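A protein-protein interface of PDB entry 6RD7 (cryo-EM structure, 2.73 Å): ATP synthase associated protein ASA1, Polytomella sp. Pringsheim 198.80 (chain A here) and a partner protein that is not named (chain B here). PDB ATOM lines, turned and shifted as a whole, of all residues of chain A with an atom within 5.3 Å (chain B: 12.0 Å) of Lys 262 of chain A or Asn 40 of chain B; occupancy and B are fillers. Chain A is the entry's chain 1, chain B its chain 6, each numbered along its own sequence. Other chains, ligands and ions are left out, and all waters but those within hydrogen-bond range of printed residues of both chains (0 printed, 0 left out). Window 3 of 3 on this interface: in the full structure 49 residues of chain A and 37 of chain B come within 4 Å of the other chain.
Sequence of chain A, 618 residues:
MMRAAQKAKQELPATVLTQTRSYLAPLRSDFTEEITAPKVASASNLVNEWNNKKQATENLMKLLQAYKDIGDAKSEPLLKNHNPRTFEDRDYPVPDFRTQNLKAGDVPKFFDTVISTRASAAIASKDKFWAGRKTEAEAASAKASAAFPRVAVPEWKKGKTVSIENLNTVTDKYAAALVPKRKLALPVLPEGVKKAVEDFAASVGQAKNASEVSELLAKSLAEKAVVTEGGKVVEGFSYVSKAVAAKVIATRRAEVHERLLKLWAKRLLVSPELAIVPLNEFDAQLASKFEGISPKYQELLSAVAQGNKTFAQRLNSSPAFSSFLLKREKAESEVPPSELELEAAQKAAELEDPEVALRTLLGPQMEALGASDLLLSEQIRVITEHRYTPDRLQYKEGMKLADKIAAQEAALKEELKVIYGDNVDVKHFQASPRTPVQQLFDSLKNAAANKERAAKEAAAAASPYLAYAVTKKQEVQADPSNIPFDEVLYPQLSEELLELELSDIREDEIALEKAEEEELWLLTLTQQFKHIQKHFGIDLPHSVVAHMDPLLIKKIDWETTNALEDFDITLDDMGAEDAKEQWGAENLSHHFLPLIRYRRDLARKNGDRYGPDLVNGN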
ATOM      1  N   HIS A 257     -27.299 -31.326   0.530  1.00  0.00           N
ATOM      2  CA  HIS A 257     -25.971 -30.840   0.891  1.00  0.00           C
ATOM      3  C   HIS A 257     -25.280 -30.174  -0.296  1.00  0.00           C
ATOM      4  O   HIS A 257     -24.532 -29.201  -0.126  1.00  0.00           O
ATOM      5  CB  HIS A 257     -25.137 -31.994   1.431  1.00  0.00           C
ATOM      6  CG  HIS A 257     -23.671 -31.718   1.456  1.00  0.00           C
ATOM      7  ND1 HIS A 257     -23.080 -30.944   2.428  1.00  0.00           N
ATOM      8  CD2 HIS A 257     -22.676 -32.108   0.626  1.00  0.00           C
ATOM      9  CE1 HIS A 257     -21.783 -30.870   2.197  1.00  0.00           C
ATOM     10  NE2 HIS A 257     -21.511 -31.566   1.109  1.00  0.00           N
ATOM     11  N   GLU A 258     -25.538 -30.672  -1.507  1.00  0.00           N
ATOM     12  CA  GLU A 258     -25.041 -30.029  -2.718  1.00  0.00           C
ATOM     13  C   GLU A 258     -25.646 -28.643  -2.898  1.00  0.00           C
ATOM     14  O   GLU A 258     -24.951 -27.700  -3.295  1.00  0.00           O
ATOM     15  CB  GLU A 258     -25.356 -30.916  -3.919  1.00  0.00           C
ATOM     16  CG  GLU A 258     -24.847 -30.425  -5.249  1.00  0.00           C
ATOM     17  CD  GLU A 258     -25.204 -31.375  -6.373  1.00  0.00           C
ATOM     18  OE1 GLU A 258     -25.872 -32.395  -6.100  1.00  0.00           O
ATOM     19  OE2 GLU A 258     -24.819 -31.107  -7.530  1.00  0.00           O
ATOM     20  N   ARG A 259     -26.939 -28.502  -2.589  1.00  0.00           N
ATOM     21  CA  ARG A 259     -27.581 -27.189  -2.631  1.00  0.00           C
ATOM     22  C   ARG A 259     -26.989 -26.235  -1.598  1.00  0.00           C
ATOM     23  O   ARG A 259     -26.823 -25.040  -1.870  1.00  0.00           O
ATOM     24  CB  ARG A 259     -29.083 -27.331  -2.413  1.00  0.00           C
ATOM     25  CG  ARG A 259     -29.798 -28.056  -3.524  1.00  0.00           C
ATOM     26  CD  ARG A 259     -29.945 -27.169  -4.737  1.00  0.00           C
ATOM     27  NE  ARG A 259     -30.730 -25.978  -4.437  1.00  0.00           N
ATOM     28  CZ  ARG A 259     -32.057 -25.927  -4.480  1.00  0.00           C
ATOM     29  NH1 ARG A 259     -32.686 -24.797  -4.194  1.00  0.00           N
ATOM     30  NH2 ARG A 259     -32.756 -27.002  -4.810  1.00  0.00           N
ATOM     31  N   LEU A 260     -26.651 -26.749  -0.412  1.00  0.00           N
ATOM     32  CA  LEU A 260     -26.027 -25.912   0.615  1.00  0.00           C
ATOM     33  C   LEU A 260     -24.635 -25.449   0.195  1.00  0.00           C
ATOM     34  O   LEU A 260     -24.268 -24.283   0.410  1.00  0.00           O
ATOM     35  CB  LEU A 260     -25.953 -26.673   1.937  1.00  0.00           C
ATOM     36  CG  LEU A 260     -25.201 -25.980   3.076  1.00  0.00           C
ATOM     37  CD1 LEU A 260     -26.001 -24.808   3.604  1.00  0.00           C
ATOM     38  CD2 LEU A 260     -24.862 -26.945   4.189  1.00  0.00           C
ATOM     39  N   LEU A 261     -23.856 -26.349  -0.413  1.00  0.00           N
ATOM     40  CA  LEU A 261     -22.523 -25.980  -0.882  1.00  0.00           C
ATOM     41  C   LEU A 261     -22.593 -24.964  -2.011  1.00  0.00           C
ATOM     42  O   LEU A 261     -21.772 -24.045  -2.069  1.00  0.00           O
ATOM     43  CB  LEU A 261     -21.749 -27.215  -1.341  1.00  0.00           C
ATOM     44  CG  LEU A 261     -21.298 -28.255  -0.317  1.00  0.00           C
ATOM     45  CD1 LEU A 261     -20.109 -29.018  -0.859  1.00  0.00           C
ATOM     46  CD2 LEU A 261     -20.954 -27.619   1.007  1.00  0.00           C
ATOM     47  N   LYS A 262     -23.582 -25.095  -2.900  1.00  0.00           N
ATOM     48  CA  LYS A 262     -23.748 -24.115  -3.969  1.00  0.00           C
ATOM     49  C   LYS A 262     -24.167 -22.757  -3.422  1.00  0.00           C
ATOM     50  O   LYS A 262     -23.700 -21.713  -3.908  1.00  0.00           O
ATOM     51  CB  LYS A 262     -24.773 -24.616  -4.978  1.00  0.00           C
ATOM     52  CG  LYS A 262     -24.257 -25.717  -5.865  1.00  0.00           C
ATOM     53  CD  LYS A 262     -25.339 -26.220  -6.787  1.00  0.00           C
ATOM     54  CE  LYS A 262     -24.863 -27.416  -7.575  1.00  0.00           C
ATOM     55  NZ  LYS A 262     -25.778 -27.730  -8.704  1.00  0.00           N
ATOM     56  N   LEU A 263     -25.031 -22.761  -2.402  1.00  0.00           N
ATOM     57  CA  LEU A 263     -25.463 -21.525  -1.761  1.00  0.00           C
ATOM     58  C   LEU A 263     -24.292 -20.786  -1.139  1.00  0.00           C
ATOM     59  O   LEU A 263     -24.128 -19.584  -1.364  1.00  0.00           O
ATOM     60  CB  LEU A 263     -26.522 -21.835  -0.706  1.00  0.00           C
ATOM     61  CG  LEU A 263     -27.265 -20.708   0.002  1.00  0.00           C
ATOM     62  CD1 LEU A 263     -28.650 -21.182   0.218  1.00  0.00           C
ATOM     63  CD2 LEU A 263     -26.655 -20.387   1.354  1.00  0.00           C
ATOM     64  N   TRP A 264     -23.458 -21.482  -0.371  1.00  0.00           N
ATOM     65  CA  TRP A 264     -22.332 -20.779   0.230  1.00  0.00           C
ATOM     66  C   TRP A 264     -21.238 -20.465  -0.782  1.00  0.00           C
ATOM     67  O   TRP A 264     -20.494 -19.496  -0.595  1.00  0.00           O
ATOM     68  CB  TRP A 264     -21.774 -21.570   1.408  1.00  0.00           C
ATOM     69  CG  TRP A 264     -22.584 -21.366   2.643  1.00  0.00           C
ATOM     70  CD1 TRP A 264     -23.356 -22.288   3.274  1.00  0.00           C
ATOM     71  CD2 TRP A 264     -22.730 -20.148   3.384  1.00  0.00           C
ATOM     72  NE1 TRP A 264     -23.964 -21.731   4.366  1.00  0.00           N
ATOM     73  CE2 TRP A 264     -23.596 -20.416   4.457  1.00  0.00           C
ATOM     74  CE3 TRP A 264     -22.207 -18.857   3.247  1.00  0.00           C
ATOM     75  CZ2 TRP A 264     -23.951 -19.446   5.387  1.00  0.00           C
ATOM     76  CZ3 TRP A 264     -22.560 -17.898   4.169  1.00  0.00           C
ATOM     77  CH2 TRP A 264     -23.425 -18.196   5.226  1.00  0.00           C
ATOM     78  N   ALA A 265     -21.161 -21.231  -1.875  1.00  0.00           N
ATOM     79  CA  ALA A 265     -20.198 -20.935  -2.926  1.00  0.00           C
ATOM     80  C   ALA A 265     -20.527 -19.626  -3.627  1.00  0.00           C
ATOM     81  O   ALA A 265     -19.618 -18.855  -3.936  1.00  0.00           O
ATOM     82  CB  ALA A 265     -20.149 -22.081  -3.931  1.00  0.00           C
ATOM     83  N   LYS A 266     -21.816 -19.346  -3.851  1.00  0.00           N
ATOM     84  CA  LYS A 266     -22.202 -18.071  -4.465  1.00  0.00           C
ATOM     85  C   LYS A 266     -21.821 -16.877  -3.591  1.00  0.00           C
ATOM     86  O   LYS A 266     -21.228 -15.902  -4.076  1.00  0.00           O
ATOM     87  CB  LYS A 266     -23.702 -18.052  -4.742  1.00  0.00           C
ATOM     88  CG  LYS A 266     -24.155 -19.015  -5.800  1.00  0.00           C
ATOM     89  CD  LYS A 266     -25.659 -19.009  -5.897  1.00  0.00           C
ATOM     90  CE  LYS A 266     -26.196 -20.384  -6.206  1.00  0.00           C
ATOM     91  NZ  LYS A 266     -27.599 -20.531  -5.751  1.00  0.00           N
ATOM     92  N   ARG A 267     -22.121 -16.954  -2.295  1.00  0.00           N
ATOM     93  CA  ARG A 267     -21.861 -15.833  -1.400  1.00  0.00           C
ATOM     94  C   ARG A 267     -20.374 -15.650  -1.141  1.00  0.00           C
ATOM     95  O   ARG A 267     -19.917 -14.530  -0.899  1.00  0.00           O
ATOM     96  CB  ARG A 267     -22.599 -16.036  -0.085  1.00  0.00           C
ATOM     97  CG  ARG A 267     -24.060 -15.718  -0.161  1.00  0.00           C
ATOM     98  CD  ARG A 267     -24.855 -16.902   0.292  1.00  0.00           C
ATOM     99  NE  ARG A 267     -26.283 -16.711   0.097  1.00  0.00           N
ATOM    100  CZ  ARG A 267     -26.927 -16.999  -1.024  1.00  0.00           C
ATOM    101  NH1 ARG A 267     -26.272 -17.492  -2.061  1.00  0.00           N
ATOM    102  NH2 ARG A 267     -28.229 -16.798  -1.105  1.00  0.00           N
ATOM    103  N   SER B  31     -22.688  -9.771 -13.395  1.00  0.00           N
ATOM    104  CA  SER B  31     -21.754 -10.847 -13.082  1.00  0.00           C
ATOM    105  C   SER B  31     -22.308 -11.781 -12.018  1.00  0.00           C
ATOM    106  O   SER B  31     -21.933 -12.956 -11.961  1.00  0.00           O
ATOM    107  CB  SER B  31     -20.420 -10.262 -12.627  1.00  0.00           C
ATOM    108  OG  SER B  31     -20.551  -9.603 -11.382  1.00  0.00           O
ATOM    109  N   VAL B  32     -23.198 -11.278 -11.165  1.00  0.00           N
ATOM    110  CA  VAL B  32     -23.724 -12.089 -10.074  1.00  0.00           C
ATOM    111  C   VAL B  32     -24.695 -13.133 -10.612  1.00  0.00           C
ATOM    112  O   VAL B  32     -24.723 -14.278 -10.149  1.00  0.00           O
ATOM    113  CB  VAL B  32     -24.374 -11.186  -9.011  1.00  0.00           C
ATOM    114  CG1 VAL B  32     -24.995 -12.002  -7.923  1.00  0.00           C
ATOM    115  CG2 VAL B  32     -23.340 -10.262  -8.420  1.00  0.00           C
ATOM    116  N   ALA B  33     -25.480 -12.763 -11.626  1.00  0.00           N
ATOM    117  CA  ALA B  33     -26.360 -13.735 -12.268  1.00  0.00           C
ATOM    118  C   ALA B  33     -25.559 -14.793 -13.012  1.00  0.00           C
ATOM    119  O   ALA B  33     -25.961 -15.959 -13.066  1.00  0.00           O
ATOM    120  CB  ALA B  33     -27.325 -13.031 -13.214  1.00  0.00           C
ATOM    121  N   GLY B  34     -24.404 -14.410 -13.560  1.00  0.00           N
ATOM    122  CA  GLY B  34     -23.510 -15.392 -14.147  1.00  0.00           C
ATOM    123  C   GLY B  34     -22.918 -16.332 -13.115  1.00  0.00           C
ATOM    124  O   GLY B  34     -22.770 -17.529 -13.374  1.00  0.00           O
ATOM    125  N   ILE B  35     -22.583 -15.803 -11.931  1.00  0.00           N
ATOM    126  CA  ILE B  35     -22.121 -16.629 -10.815  1.00  0.00           C
ATOM    127  C   ILE B  35     -23.195 -17.627 -10.411  1.00  0.00           C
ATOM    128  O   ILE B  35     -22.924 -18.823 -10.270  1.00  0.00           O
ATOM    129  CB  ILE B  35     -21.713 -15.747  -9.620  1.00  0.00           C
ATOM    130  CG1 ILE B  35     -20.358 -15.099  -9.846  1.00  0.00           C
ATOM    131  CG2 ILE B  35     -21.660 -16.547  -8.324  1.00  0.00           C
ATOM    132  CD1 ILE B  35     -19.957 -14.165  -8.725  1.00  0.00           C
ATOM    133  N   ILE B  36     -24.430 -17.147 -10.246  1.00  0.00           N
ATOM    134  CA  ILE B  36     -25.547 -17.984  -9.811  1.00  0.00           C
ATOM    135  C   ILE B  36     -25.835 -19.073 -10.836  1.00  0.00           C
ATOM    136  O   ILE B  36     -25.973 -20.251 -10.484  1.00  0.00           O
ATOM    137  CB  ILE B  36     -26.782 -17.103  -9.545  1.00  0.00           C
ATOM    138  CG1 ILE B  36     -26.576 -16.273  -8.280  1.00  0.00           C
ATOM    139  CG2 ILE B  36     -28.041 -17.937  -9.428  1.00  0.00           C
ATOM    140  CD1 ILE B  36     -27.588 -15.173  -8.106  1.00  0.00           C
ATOM    141  N   LYS B  37     -25.845 -18.709 -12.122  1.00  0.00           N
ATOM    142  CA  LYS B  37     -26.098 -19.672 -13.188  1.00  0.00           C
ATOM    143  C   LYS B  37     -24.997 -20.721 -13.280  1.00  0.00           C
ATOM    144  O   LYS B  37     -25.285 -21.923 -13.300  1.00  0.00           O
ATOM    145  CB  LYS B  37     -26.238 -18.940 -14.518  1.00  0.00           C
ATOM    146  CG  LYS B  37     -27.173 -19.600 -15.501  1.00  0.00           C
ATOM    147  CD  LYS B  37     -27.214 -18.824 -16.800  1.00  0.00           C
ATOM    148  CE  LYS B  37     -27.348 -19.751 -17.989  1.00  0.00           C
ATOM    149  NZ  LYS B  37     -28.620 -20.517 -17.937  1.00  0.00           N
ATOM    150  N   SER B  38     -23.732 -20.300 -13.298  1.00  0.00           N
ATOM    151  CA  SER B  38     -22.661 -21.261 -13.519  1.00  0.00           C
ATOM    152  C   SER B  38     -22.342 -22.058 -12.260  1.00  0.00           C
ATOM    153  O   SER B  38     -21.726 -23.123 -12.345  1.00  0.00           O
ATOM    154  CB  SER B  38     -21.420 -20.547 -14.041  1.00  0.00           C
ATOM    155  OG  SER B  38     -20.950 -19.617 -13.095  1.00  0.00           O
ATOM    156  N   VAL B  39     -22.748 -21.574 -11.085  1.00  0.00           N
ATOM    157  CA  VAL B  39     -22.627 -22.390  -9.883  1.00  0.00           C
ATOM    158  C   VAL B  39     -23.758 -23.407  -9.825  1.00  0.00           C
ATOM    159  O   VAL B  39     -23.544 -24.574  -9.470  1.00  0.00           O
ATOM    160  CB  VAL B  39     -22.569 -21.487  -8.632  1.00  0.00           C
ATOM    161  CG1 VAL B  39     -22.961 -22.230  -7.367  1.00  0.00           C
ATOM    162  CG2 VAL B  39     -21.170 -20.932  -8.460  1.00  0.00           C
ATOM    163  N   ASN B  40     -24.963 -23.009 -10.249  1.00  0.00           N
ATOM    164  CA  ASN B  40     -26.082 -23.943 -10.288  1.00  0.00           C
ATOM    165  C   ASN B  40     -25.900 -25.002 -11.371  1.00  0.00           C
ATOM    166  O   ASN B  40     -26.487 -26.086 -11.291  1.00  0.00           O
ATOM    167  CB  ASN B  40     -27.385 -23.180 -10.510  1.00  0.00           C
ATOM    168  CG  ASN B  40     -27.906 -22.539  -9.247  1.00  0.00           C
ATOM    169  OD1 ASN B  40     -28.787 -21.683  -9.294  1.00  0.00           O
ATOM    170  ND2 ASN B  40     -27.372 -22.951  -8.109  1.00  0.00           N
ATOM    171  N   GLU B  41     -25.094 -24.709 -12.395  1.00  0.00           N
ATOM    172  CA  GLU B  41     -24.938 -25.657 -13.494  1.00  0.00           C
ATOM    173  C   GLU B  41     -23.908 -26.737 -13.183  1.00  0.00           C
ATOM    174  O   GLU B  41     -23.909 -27.795 -13.823  1.00  0.00           O
ATOM    175  CB  GLU B  41     -24.557 -24.924 -14.776  1.00  0.00           C
ATOM    176  CG  GLU B  41     -25.724 -24.287 -15.496  1.00  0.00           C
ATOM    177  CD  GLU B  41     -25.277 -23.402 -16.637  1.00  0.00           C
ATOM    178  OE1 GLU B  41     -24.053 -23.227 -16.811  1.00  0.00           O
ATOM    179  OE2 GLU B  41     -26.149 -22.873 -17.356  1.00  0.00           O
ATOM    180  N   THR B  42     -23.008 -26.496 -12.232  1.00  0.00           N
ATOM    181  CA  THR B  42     -22.010 -27.505 -11.900  1.00  0.00           C
ATOM    182  C   THR B  42     -22.637 -28.650 -11.120  1.00  0.00           C
ATOM    183  O   THR B  42     -23.640 -28.476 -10.427  1.00  0.00           O
ATOM    184  CB  THR B  42     -20.861 -26.908 -11.085  1.00  0.00           C
ATOM    185  OG1 THR B  42     -21.376 -26.283  -9.904  1.00  0.00           O
ATOM    186  CG2 THR B  42     -20.070 -25.910 -11.899  1.00  0.00           C
ATOM    187  N   SER B  43     -22.048 -29.831 -11.251  1.00  0.00           N
ATOM    188  CA  SER B  43     -22.409 -30.936 -10.385  1.00  0.00           C
ATOM    189  C   SER B  43     -21.675 -30.803  -9.057  1.00  0.00           C
ATOM    190  O   SER B  43     -20.820 -29.932  -8.879  1.00  0.00           O
ATOM    191  CB  SER B  43     -22.083 -32.274 -11.046  1.00  0.00           C
ATOM    192  OG  SER B  43     -20.685 -32.449 -11.186  1.00  0.00           O
ATOM    193  N   GLY B  44     -22.028 -31.677  -8.114  1.00  0.00           N
ATOM    194  CA  GLY B  44     -21.403 -31.622  -6.802  1.00  0.00           C
ATOM    195  C   GLY B  44     -19.943 -32.031  -6.828  1.00  0.00           C
ATOM    196  O   GLY B  44     -19.135 -31.538  -6.038  1.00  0.00           O
ATOM    197  N   ALA B  45     -19.584 -32.931  -7.744  1.00  0.00           N
ATOM    198  CA  ALA B  45     -18.187 -33.329  -7.877  1.00  0.00           C
ATOM    199  C   ALA B  45     -17.386 -32.279  -8.633  1.00  0.00           C
ATOM    200  O   ALA B  45     -16.191 -32.095  -8.380  1.00  0.00           O
ATOM    201  CB  ALA B  45     -18.097 -34.683  -8.578  1.00  0.00           C
ATOM    202  N   ASN B  46     -18.027 -31.578  -9.563  1.00  0.00           N
ATOM    203  CA  ASN B  46     -17.371 -30.572 -10.386  1.00  0.00           C
ATOM    204  C   ASN B  46     -17.278 -29.212  -9.713  1.00  0.00           C
ATOM    205  O   ASN B  46     -16.654 -28.310 -10.276  1.00  0.00           O
ATOM    206  CB  ASN B  46     -18.121 -30.409 -11.712  1.00  0.00           C
ATOM    207  CG  ASN B  46     -17.576 -31.296 -12.805  1.00  0.00           C
ATOM    208  OD1 ASN B  46     -16.492 -31.863 -12.681  1.00  0.00           O
ATOM    209  ND2 ASN B  46     -18.329 -31.420 -13.891  1.00  0.00           N
ATOM    210  N   LEU B  47     -17.871 -29.046  -8.528  1.00  0.00           N
ATOM    211  CA  LEU B  47     -18.136 -27.708  -8.006  1.00  0.00           C
ATOM    212  C   LEU B  47     -16.872 -27.022  -7.509  1.00  0.00           C
ATOM    213  O   LEU B  47     -16.603 -25.871  -7.869  1.00  0.00           O
ATOM    214  CB  LEU B  47     -19.168 -27.775  -6.882  1.00  0.00           C
ATOM    215  CG  LEU B  47     -19.320 -26.503  -6.044  1.00  0.00           C
ATOM    216  CD1 LEU B  47     -20.016 -25.417  -6.842  1.00  0.00           C
ATOM    217  CD2 LEU B  47     -20.067 -26.785  -4.757  1.00  0.00           C
ATOM    218  N   LEU B  48     -16.077 -27.714  -6.693  1.00  0.00           N
ATOM    219  CA  LEU B  48     -15.043 -27.035  -5.918  1.00  0.00           C
ATOM    220  C   LEU B  48     -13.848 -26.649  -6.777  1.00  0.00           C
ATOM    221  O   LEU B  48     -13.133 -25.693  -6.460  1.00  0.00           O
ATOM    222  CB  LEU B  48     -14.599 -27.913  -4.753  1.00  0.00           C
ATOM    223  CG  LEU B  48     -15.391 -27.817  -3.450  1.00  0.00           C
ATOM    224  CD1 LEU B  48     -16.703 -28.580  -3.515  1.00  0.00           C
ATOM    225  CD2 LEU B  48     -14.537 -28.333  -2.319  1.00  0.00           C
ATOM    226  N   SER B  49     -13.610 -27.376  -7.868  1.00  0.00           N
ATOM    227  CA  SER B  49     -12.487 -27.031  -8.733  1.00  0.00           C
ATOM    228  C   SER B  49     -12.894 -26.009  -9.784  1.00  0.00           C
ATOM    229  O   SER B  49     -12.039 -25.326 -10.358  1.00  0.00           O
ATOM    230  CB  SER B  49     -11.926 -28.287  -9.391  1.00  0.00           C
ATOM    231  OG  SER B  49     -12.630 -28.591 -10.578  1.00  0.00           O
ATOM    232  N   SER B  50     -14.190 -25.885 -10.051  1.00  0.00           N
ATOM    233  CA  SER B  50     -14.688 -24.888 -10.988  1.00  0.00           C
ATOM    234  C   SER B  50     -14.739 -23.489 -10.393  1.00  0.00           C
ATOM    235  O   SER B  50     -14.899 -22.522 -11.148  1.00  0.00           O
ATOM    236  CB  SER B  50     -16.082 -25.284 -11.476  1.00  0.00           C
ATOM    237  OG  SER B  50     -17.015 -25.254 -10.412  1.00  0.00           O
ATOM    238  N   LEU B  51     -14.573 -23.366  -9.074  1.00  0.00           N
ATOM    239  CA  LEU B  51     -14.839 -22.110  -8.381  1.00  0.00           C
ATOM    240  C   LEU B  51     -13.829 -21.031  -8.743  1.00  0.00           C
ATOM    241  O   LEU B  51     -14.153 -19.839  -8.715  1.00  0.00           O
ATOM    242  CB  LEU B  51     -14.833 -22.346  -6.877  1.00  0.00           C
ATOM    243  CG  LEU B  51     -16.059 -22.943  -6.200  1.00  0.00           C
ATOM    244  CD1 LEU B  51     -15.940 -22.675  -4.731  1.00  0.00           C
ATOM    245  CD2 LEU B  51     -17.338 -22.355  -6.746  1.00  0.00           C
ATOM    246  N   THR B  53     -12.564 -20.820 -11.753  1.00  0.00           N
ATOM    247  CA  THR B  53     -12.897 -20.411 -13.110  1.00  0.00           C
ATOM    248  C   THR B  53     -14.062 -19.435 -13.107  1.00  0.00           C
ATOM    249  O   THR B  53     -13.996 -18.385 -13.758  1.00  0.00           O
ATOM    250  CB  THR B  53     -13.221 -21.638 -13.961  1.00  0.00           C
ATOM    251  OG1 THR B  53     -12.079 -22.500 -14.002  1.00  0.00           O
ATOM    252  CG2 THR B  53     -13.591 -21.233 -15.375  1.00  0.00           C
ATOM    253  N   ILE B  54     -15.110 -19.770 -12.345  1.00  0.00           N
ATOM    254  CA  ILE B  54     -16.311 -18.946 -12.227  1.00  0.00           C
ATOM    255  C   ILE B  54     -15.965 -17.563 -11.697  1.00  0.00           C
ATOM    256  O   ILE B  54     -16.426 -16.545 -12.233  1.00  0.00           O
ATOM    257  CB  ILE B  54     -17.337 -19.657 -11.327  1.00  0.00           C
ATOM    258  CG1 ILE B  54     -17.775 -20.975 -11.960  1.00  0.00           C
ATOM    259  CG2 ILE B  54     -18.531 -18.775 -11.069  1.00  0.00           C
ATOM    260  CD1 ILE B  54     -18.577 -21.847 -11.040  1.00  0.00           C
ATOM    261  N   LYS B  55     -15.108 -17.514 -10.670  1.00  0.00           N
ATOM    262  CA  LYS B  55     -14.587 -16.258 -10.141  1.00  0.00           C
ATOM    263  C   LYS B  55     -13.881 -15.447 -11.216  1.00  0.00           C
ATOM    264  O   LYS B  55     -14.094 -14.233 -11.326  1.00  0.00           O
ATOM    265  CB  LYS B  55     -13.623 -16.547  -8.994  1.00  0.00           C
ATOM    266  CG  LYS B  55     -13.150 -15.326  -8.251  1.00  0.00           C
ATOM    267  CD  LYS B  55     -12.192 -15.711  -7.146  1.00  0.00           C
ATOM    268  CE  LYS B  55     -11.678 -14.481  -6.428  1.00  0.00           C
ATOM    269  NZ  LYS B  55     -12.786 -13.753  -5.755  1.00  0.00           N
ATOM    270  N   GLN B  57     -14.514 -15.516 -14.300  1.00  0.00           N
ATOM    271  CA  GLN B  57     -15.480 -15.012 -15.266  1.00  0.00           C
ATOM    272  C   GLN B  57     -16.337 -13.916 -14.651  1.00  0.00           C
ATOM    273  O   GLN B  57     -17.097 -13.242 -15.355  1.00  0.00           O
ATOM    274  CB  GLN B  57     -16.345 -16.152 -15.793  1.00  0.00           C
ATOM    275  CG  GLN B  57     -15.548 -17.230 -16.498  1.00  0.00           C
ATOM    276  CD  GLN B  57     -16.389 -18.430 -16.865  1.00  0.00           C
ATOM    277  OE1 GLN B  57     -16.944 -19.103 -15.997  1.00  0.00           O
ATOM    278  NE2 GLN B  57     -16.485 -18.712 -18.159  1.00  0.00           N
ATOM    279  N   SER B 150     -26.734 -12.349   2.669  1.00  0.00           N
ATOM    280  CA  SER B 150     -27.781 -13.160   2.070  1.00  0.00           C
ATOM    281  C   SER B 150     -27.679 -14.585   2.589  1.00  0.00           C
ATOM    282  O   SER B 150     -26.664 -15.248   2.371  1.00  0.00           O
ATOM    283  CB  SER B 150     -27.673 -13.153   0.544  1.00  0.00           C
ATOM    284  OG  SER B 150     -28.656 -13.993  -0.031  1.00  0.00           O
ATOM    285  N   LEU B 151     -28.716 -15.029   3.298  1.00  0.00           N
ATOM    286  CA  LEU B 151     -28.937 -16.440   3.630  1.00  0.00           C
ATOM    287  C   LEU B 151     -30.385 -16.604   4.083  1.00  0.00           C
ATOM    288  O   LEU B 151     -30.798 -17.678   4.514  1.00  0.00           O
ATOM    289  CB  LEU B 151     -27.962 -16.948   4.708  1.00  0.00           C
ATOM    290  CG  LEU B 151     -27.916 -16.436   6.150  1.00  0.00           C
ATOM    291  CD1 LEU B 151     -28.753 -17.294   7.088  1.00  0.00           C
ATOM    292  CD2 LEU B 151     -26.489 -16.380   6.641  1.00  0.00           C
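OE2 of Glu 258 of chain A lies within salt-bridge range of NZ of Lys 262 of chain A (3.7 Å).
O of Leu 263 of chain A is in hydrogen-bond range of NH1 of Arg 267 of chain A (3.1 Å).
O of Ile 36 of chain B sits close to OD1 of Asn 40 of chain B (3.4 Å).
The side-chain hydroxyl (OG1) of Thr 42 of chain B is in hydrogen-bond range of the backbone carbonyl oxygen (O) of Val 39 of chain B, at 2.8 Å.
Asn 40 of chain B touches just these residues of chain A: Lys 262 (3.1 Å) and Lys 266 (3.4 Å).
Of the printed residues of chain B, Glu 258 of chain A touches Ser 43 and Gly 44.
No residue of chain B comes within 4 Å of Arg 259 of chain A.
No residue of chain B comes within 4 Å of Leu 260 of chain A.
Of the printed residues of chain B, Leu 261 of chain A touches Leu 47.
No residue of chain B comes within 4 Å of Leu 263 of chain A.
Lys 266 of chain A touches just these residues of chain B: Ile 36, Val 39 and Asn 40.
Of the printed residues of chain B, Ala 265 of chain A touches Leu 51.
Of the printed residues of chain A, Leu 51 of chain B touches Ala 265 (3.99 Å).
Printed residues of chain A within 4 Å of Gly 44 of chain B: Glu 258.
Printed residues of chain A within 4 Å of Leu 47 of chain B: Leu 261.
Of the printed residues of chain A, Thr 42 of chain B touches Lys 262 (2.8 Å).
The nearest printed residue of chain A that does not touch Asn 40 of chain B is Arg 259 of chain A (5.8 Å).
Ser 43 of chain B touches Glu 258 of chain A.
Leu 261 of chain A touches Leu 47 of chain B.
O of Lys 262 of chain A touches CG1 of Val 39 of chain B (3.6 Å).
Leu 151 of chain B touches Trp 264 of chain A (CD2 to CH2, 3.8 Å).
CB of Ala 265 of chain A touches CD2 of Leu 51 of chain B, 3.99 Å away.
Ile 36 of chain B touches Lys 266 of chain A.
CG1 of Val 39 of chain B touches CG of Lys 266 of chain A, 3.8 Å away.
The side-chain carboxylate of Glu 258 of chain A sits at hydrogen-bond distance from the backbone NH of Gly 44 of chain B.
The backbone carbonyl oxygen (O) of Asn 40 of chain B is in hydrogen-bond range of the side-chain amino group (NZ) of Lys 262 of chain A.
NZ of Lys 262 of chain A is in hydrogen-bond range of O of Thr 42 of chain B, 2.8 Å away.
ND2 of Asn 40 of chain B sits close to NZ of Lys 266 of chain A (3.4 Å).
The guanidinium group of Arg 267 of chain A is in hydrogen-bond range of the backbone carbonyl oxygen of Ser 150 of chain B (2.7 Å).
Hydrophobic or aromatic side chains of chain B within 4 Å of the printed part of chain A: Ile 36, Val 39, Leu 47, Leu 51 and Leu 151.
Of the 11 printed residues of chain A, 7 touch a printed residue of chain B.
Printed residues of chain A that touch a printed residue of chain B: Glu 258, Leu 261, Lys 262, Trp 264, Ala 265, Lys 266 and Arg 267.
Hydrophobic or aromatic side chains of chain A that line the printed part of chain B: Leu 261, Trp 264 and Ala 265.
Among the printed residues, 12 pairs touch across the chains.
Among the printed residues, no Asp or Glu carboxylate lies within 4 Å of a Lys or Arg side-chain nitrogen of the other chain.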
